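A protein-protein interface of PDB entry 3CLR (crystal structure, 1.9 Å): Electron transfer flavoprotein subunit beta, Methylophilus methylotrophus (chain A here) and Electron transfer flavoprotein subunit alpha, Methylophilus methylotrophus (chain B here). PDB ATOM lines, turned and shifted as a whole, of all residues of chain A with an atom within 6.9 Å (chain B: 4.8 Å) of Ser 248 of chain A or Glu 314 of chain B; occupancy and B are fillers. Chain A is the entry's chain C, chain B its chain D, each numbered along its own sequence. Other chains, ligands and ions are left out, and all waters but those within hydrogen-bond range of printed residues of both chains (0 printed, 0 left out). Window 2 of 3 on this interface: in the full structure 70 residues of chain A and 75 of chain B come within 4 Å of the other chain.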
ATOM      1  N   GLY A 245       6.523  16.157  26.324  1.00  0.00           N
ATOM      2  CA  GLY A 245       7.531  15.359  27.014  1.00  0.00           C
ATOM      3  C   GLY A 245       8.887  15.632  26.421  1.00  0.00           C
ATOM      4  O   GLY A 245       9.102  16.686  25.837  1.00  0.00           O
ATOM      5  N   THR A 246       9.796  14.671  26.568  1.00  0.00           N
ATOM      6  CA  THR A 246      11.188  14.855  26.172  1.00  0.00           C
ATOM      7  C   THR A 246      11.425  14.732  24.681  1.00  0.00           C
ATOM      8  O   THR A 246      10.623  14.177  23.930  1.00  0.00           O
ATOM      9  CB  THR A 246      12.127  13.850  26.879  1.00  0.00           C
ATOM     10  OG1 THR A 246      11.922  12.528  26.366  1.00  0.00           O
ATOM     11  CG2 THR A 246      11.888  13.862  28.374  1.00  0.00           C
ATOM     12  N   ILE A 247      12.556  15.275  24.267  1.00  0.00           N
ATOM     13  CA  ILE A 247      13.033  15.108  22.920  1.00  0.00           C
ATOM     14  C   ILE A 247      13.080  13.632  22.562  1.00  0.00           C
ATOM     15  O   ILE A 247      12.644  13.241  21.488  1.00  0.00           O
ATOM     16  CB  ILE A 247      14.389  15.777  22.782  1.00  0.00           C
ATOM     17  CG1 ILE A 247      14.183  17.303  22.776  1.00  0.00           C
ATOM     18  CG2 ILE A 247      15.138  15.233  21.573  1.00  0.00           C
ATOM     19  CD1 ILE A 247      13.513  17.870  21.524  1.00  0.00           C
ATOM     20  N   SER A 248      13.535  12.802  23.490  1.00  0.00           N
ATOM     21  CA  SER A 248      13.562  11.366  23.234  1.00  0.00           C
ATOM     22  C   SER A 248      12.155  10.752  23.043  1.00  0.00           C
ATOM     23  O   SER A 248      11.951   9.922  22.160  1.00  0.00           O
ATOM     24  CB  SER A 248      14.350  10.647  24.330  1.00  0.00           C
ATOM     25  OG  SER A 248      14.049   9.273  24.353  1.00  0.00           O
ATOM     26  N   GLU A 249      11.195  11.152  23.875  1.00  0.00           N
ATOM     27  CA  GLU A 249       9.828  10.646  23.776  1.00  0.00           C
ATOM     28  C   GLU A 249       9.190  11.161  22.486  1.00  0.00           C
ATOM     29  O   GLU A 249       8.485  10.411  21.818  1.00  0.00           O
ATOM     30  CB  GLU A 249       8.967  11.062  24.990  1.00  0.00           C
ATOM     31  CG  GLU A 249       9.411  10.476  26.324  1.00  0.00           C
ATOM     32  CD  GLU A 249       8.812  11.183  27.540  1.00  0.00           C
ATOM     33  OE1 GLU A 249       8.482  12.379  27.501  1.00  0.00           O
ATOM     34  OE2 GLU A 249       8.666  10.530  28.586  1.00  0.00           O
ATOM     35  N   GLN A 250       9.443  12.429  22.134  1.00  0.00           N
ATOM     36  CA  GLN A 250       8.904  13.013  20.902  1.00  0.00           C
ATOM     37  C   GLN A 250       9.469  12.299  19.693  1.00  0.00           C
ATOM     38  O   GLN A 250       8.724  11.902  18.789  1.00  0.00           O
ATOM     39  CB  GLN A 250       9.184  14.514  20.834  1.00  0.00           C
ATOM     40  CG  GLN A 250       8.330  15.303  21.807  1.00  0.00           C
ATOM     41  CD  GLN A 250       8.806  16.692  22.093  1.00  0.00           C
ATOM     42  OE1 GLN A 250      10.005  16.996  22.066  1.00  0.00           O
ATOM     43  NE2 GLN A 250       7.850  17.570  22.399  1.00  0.00           N
ATOM     44  N   ALA A 251      10.787  12.099  19.666  1.00  0.00           N
ATOM     45  CA  ALA A 251      11.412  11.326  18.584  1.00  0.00           C
ATOM     46  C   ALA A 251      10.918   9.870  18.494  1.00  0.00           C
ATOM     47  O   ALA A 251      10.797   9.316  17.394  1.00  0.00           O
ATOM     48  CB  ALA A 251      12.935  11.367  18.707  1.00  0.00           C
ATOM     49  N   ALA A 252      10.675   9.232  19.644  1.00  0.00           N
ATOM     50  CA  ALA A 252      10.207   7.854  19.664  1.00  0.00           C
ATOM     51  C   ALA A 252       8.812   7.749  19.027  1.00  0.00           C
ATOM     52  O   ALA A 252       8.524   6.780  18.296  1.00  0.00           O
ATOM     53  CB  ALA A 252      10.195   7.310  21.090  1.00  0.00           C
ATOM     54  N   LYS A 253       7.959   8.743  19.287  1.00  0.00           N
ATOM     55  CA  LYS A 253       6.628   8.771  18.693  1.00  0.00           C
ATOM     56  C   LYS A 253       6.680   8.969  17.175  1.00  0.00           C
ATOM     57  O   LYS A 253       5.970   8.306  16.462  1.00  0.00           O
ATOM     58  CB  LYS A 253       5.731   9.829  19.355  1.00  0.00           C
ATOM     59  CG  LYS A 253       4.280   9.881  18.778  1.00  0.00           C
ATOM     60  CD  LYS A 253       3.536   8.560  18.838  1.00  0.00           C
ATOM     61  CE  LYS A 253       2.153   8.707  18.268  1.00  0.00           C
ATOM     62  NZ  LYS A 253       1.305   7.459  18.321  1.00  0.00           N
ATOM     63  N   ILE A 255       9.068   7.979  15.297  1.00  0.00           N
ATOM     64  CA  ILE A 255       9.523   6.738  14.699  1.00  0.00           C
ATOM     65  C   ILE A 255       8.379   5.682  14.675  1.00  0.00           C
ATOM     66  O   ILE A 255       8.254   4.937  13.705  1.00  0.00           O
ATOM     67  CB  ILE A 255      10.819   6.248  15.365  1.00  0.00           C
ATOM     68  CG1 ILE A 255      11.955   7.197  14.967  1.00  0.00           C
ATOM     69  CG2 ILE A 255      11.122   4.804  14.951  1.00  0.00           C
ATOM     70  CD1 ILE A 255      13.285   6.963  15.651  1.00  0.00           C
ATOM     71  N   ASP B 310      17.587  19.461  17.683  1.00  0.00           N
ATOM     72  CA  ASP B 310      17.503  18.458  18.760  1.00  0.00           C
ATOM     73  C   ASP B 310      16.702  17.234  18.327  1.00  0.00           C
ATOM     74  O   ASP B 310      17.099  16.103  18.587  1.00  0.00           O
ATOM     75  CB  ASP B 310      16.868  19.057  20.021  1.00  0.00           C
ATOM     76  CG  ASP B 310      17.756  20.101  20.677  1.00  0.00           C
ATOM     77  OD1 ASP B 310      18.916  20.157  20.307  1.00  0.00           O
ATOM     78  OD2 ASP B 310      17.305  20.855  21.561  1.00  0.00           O
ATOM     79  N   ILE B 311      15.584  17.465  17.662  1.00  0.00           N
ATOM     80  CA  ILE B 311      14.736  16.368  17.192  1.00  0.00           C
ATOM     81  C   ILE B 311      15.487  15.544  16.142  1.00  0.00           C
ATOM     82  O   ILE B 311      15.574  14.326  16.245  1.00  0.00           O
ATOM     83  CB  ILE B 311      13.366  16.891  16.660  1.00  0.00           C
ATOM     84  CG1 ILE B 311      12.477  17.374  17.841  1.00  0.00           C
ATOM     85  CG2 ILE B 311      12.653  15.842  15.812  1.00  0.00           C
ATOM     86  CD1 ILE B 311      11.856  16.253  18.738  1.00  0.00           C
ATOM     87  N   GLU B 312      16.037  16.207  15.137  1.00  0.00           N
ATOM     88  CA  GLU B 312      16.791  15.514  14.095  1.00  0.00           C
ATOM     89  C   GLU B 312      17.928  14.642  14.657  1.00  0.00           C
ATOM     90  O   GLU B 312      18.112  13.499  14.232  1.00  0.00           O
ATOM     91  CB  GLU B 312      17.336  16.538  13.085  1.00  0.00           C
ATOM     92  CG  GLU B 312      18.342  15.972  12.080  1.00  0.00           C
ATOM     93  CD  GLU B 312      19.783  16.022  12.571  1.00  0.00           C
ATOM     94  OE1 GLU B 312      20.198  17.046  13.155  1.00  0.00           O
ATOM     95  OE2 GLU B 312      20.507  15.030  12.377  1.00  0.00           O
ATOM     96  N   GLU B 313      18.724  15.185  15.574  1.00  0.00           N
ATOM     97  CA  GLU B 313      19.828  14.397  16.113  1.00  0.00           C
ATOM     98  C   GLU B 313      19.330  13.185  16.918  1.00  0.00           C
ATOM     99  O   GLU B 313      19.910  12.100  16.817  1.00  0.00           O
ATOM    100  CB  GLU B 313      20.844  15.242  16.878  1.00  0.00           C
ATOM    101  CG  GLU B 313      20.380  15.750  18.194  1.00  0.00           C
ATOM    102  CD  GLU B 313      21.520  16.185  19.133  1.00  0.00           C
ATOM    103  OE1 GLU B 313      22.599  15.524  19.180  1.00  0.00           O
ATOM    104  OE2 GLU B 313      21.315  17.204  19.841  1.00  0.00           O
ATOM    105  N   GLU B 314      18.228  13.357  17.654  1.00  0.00           N
ATOM    106  CA  GLU B 314      17.658  12.268  18.455  1.00  0.00           C
ATOM    107  C   GLU B 314      17.005  11.231  17.551  1.00  0.00           C
ATOM    108  O   GLU B 314      17.137  10.022  17.775  1.00  0.00           O
ATOM    109  CB  GLU B 314      16.665  12.812  19.475  1.00  0.00           C
ATOM    110  CG  GLU B 314      16.026  11.781  20.390  1.00  0.00           C
ATOM    111  CD  GLU B 314      17.017  11.054  21.260  1.00  0.00           C
ATOM    112  OE1 GLU B 314      18.079  11.629  21.611  1.00  0.00           O
ATOM    113  OE2 GLU B 314      16.733   9.892  21.607  1.00  0.00           O
ATOM    114  N   LEU B 315      16.327  11.694  16.509  1.00  0.00           N
ATOM    115  CA  LEU B 315      15.765  10.786  15.509  1.00  0.00           C
ATOM    116  C   LEU B 315      16.868   9.950  14.854  1.00  0.00           C
ATOM    117  O   LEU B 315      16.753   8.715  14.752  1.00  0.00           O
ATOM    118  CB  LEU B 315      15.049  11.620  14.457  1.00  0.00           C
ATOM    119  CG  LEU B 315      13.668  11.371  13.922  1.00  0.00           C
ATOM    120  CD1 LEU B 315      12.692  10.635  14.851  1.00  0.00           C
ATOM    121  CD2 LEU B 315      13.152  12.729  13.457  1.00  0.00           C
ATOM    122  N   LYS B 316      17.939  10.622  14.433  1.00  0.00           N
ATOM    123  CA  LYS B 316      19.092   9.957  13.828  1.00  0.00           C
ATOM    124  C   LYS B 316      19.681   8.893  14.746  1.00  0.00           C
ATOM    125  O   LYS B 316      19.999   7.789  14.284  1.00  0.00           O
ATOM    126  CB  LYS B 316      20.198  10.970  13.445  1.00  0.00           C
ATOM    127  N   ALA B 317      19.826   9.216  16.030  1.00  0.00           N
ATOM    128  CA  ALA B 317      20.343   8.256  17.003  1.00  0.00           C
ATOM    129  C   ALA B 317      19.429   7.047  17.165  1.00  0.00           C
ATOM    130  O   ALA B 317      19.884   5.897  17.077  1.00  0.00           O
ATOM    131  CB  ALA B 317      20.556   8.918  18.341  1.00  0.00           C
ATOM    132  N   GLN B 318      18.154   7.313  17.423  1.00  0.00           N
ATOM    133  CA  GLN B 318      17.161   6.263  17.557  1.00  0.00           C
ATOM    134  C   GLN B 318      17.072   5.388  16.318  1.00  0.00           C
ATOM    135  O   GLN B 318      16.971   4.164  16.443  1.00  0.00           O
ATOM    136  CB  GLN B 318      15.789   6.833  17.914  1.00  0.00           C
ATOM    137  CG  GLN B 318      15.762   7.384  19.320  1.00  0.00           C
ATOM    138  CD  GLN B 318      14.397   7.679  19.846  1.00  0.00           C
ATOM    139  OE1 GLN B 318      13.394   7.108  19.399  1.00  0.00           O
ATOM    140  NE2 GLN B 318      14.339   8.574  20.829  1.00  0.00           N
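Ile 247 of chain A touches Asp 310 of chain B. Ile 247 of chain A touches Ile 311 of chain B (CD1 to CD1, 3.6 Å). Ile 247 of chain A touches Glu 314 of chain B (CG2 to CB, 3.5 Å). Glu 314 of chain B touches Ser 248 of chain A. Ile 311 of chain B touches Gln 250 of chain A. Ala 251 of chain A touches Glu 314 of chain B. Ala 251 of chain A touches Leu 315 of chain B (O to CD1, 3.4 Å). CB of Ala 251 of chain A touches NE2 of Gln 318 of chain B (3.8 Å). Leu 315 of chain B touches Ile 255 of chain A (CD1 to CG1, 3.5 Å). Ile 255 of chain A touches Gln 318 of chain B.
Glu 314 of chain B touches just these residues of chain A: Ile 247, Ser 248 and Ala 251. Printed residues of chain B within 4 Å of Gln 250 of chain A: Ile 311. Printed residues of chain A within 4 Å of Gln 318 of chain B: Ser 248, Ala 251, Ala 252 and Ile 255. Of the printed residues of chain B, Ala 252 of chain A touches Gln 318. Glu 312 of chain B touches none of the printed residues of chain A. Thr 246 of chain A touches none of the printed residues of chain B. The nearest printed residue of chain A that does not touch Gln 318 of chain B is Ile 247 of chain A (5.0 Å).
Printed residues of chain A that touch a printed residue of chain B: Ile 247, Ser 248, Gln 250, Ala 251, Ala 252 and Ile 255. Hydrophobic or aromatic side chains of chain A within 4 Å of the printed part of chain B: Ile 247, Ala 251, Ala 252 and Ile 255. Printed residues of chain B that touch a printed residue of chain A: Asp 310, Ile 311, Glu 314, Leu 315 and Gln 318. Hydrophobic or aromatic side chains of chain B that line the printed part of chain A: Ile 311 and Leu 315. Among the printed residues, no Asp or Glu carboxylate lies within 4 Å of a Lys or Arg side-chain nitrogen of the other chain.
N of Ala 252 of chain A lies close to OE1 of Gln 318 of chain B. NE2 of Gln 318 of chain B sits at hydrogen-bond distance from O of Ser 248 of chain A (3.0 Å).
The side-chain amide nitrogen of Gln 318 of chain B is in hydrogen-bond range of the side-chain carboxylate of Glu 314 of chain B, at 2.8 Å. The backbone carbonyl oxygen (O) of Thr 246 of chain A lies close to the side-chain amide oxygen (OE1) of Gln 250 of chain A (3.4 Å). The backbone NH (N) of Ser 248 of chain A lies close to the side-chain hydroxyl (OG1) of Thr 246 of chain A.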
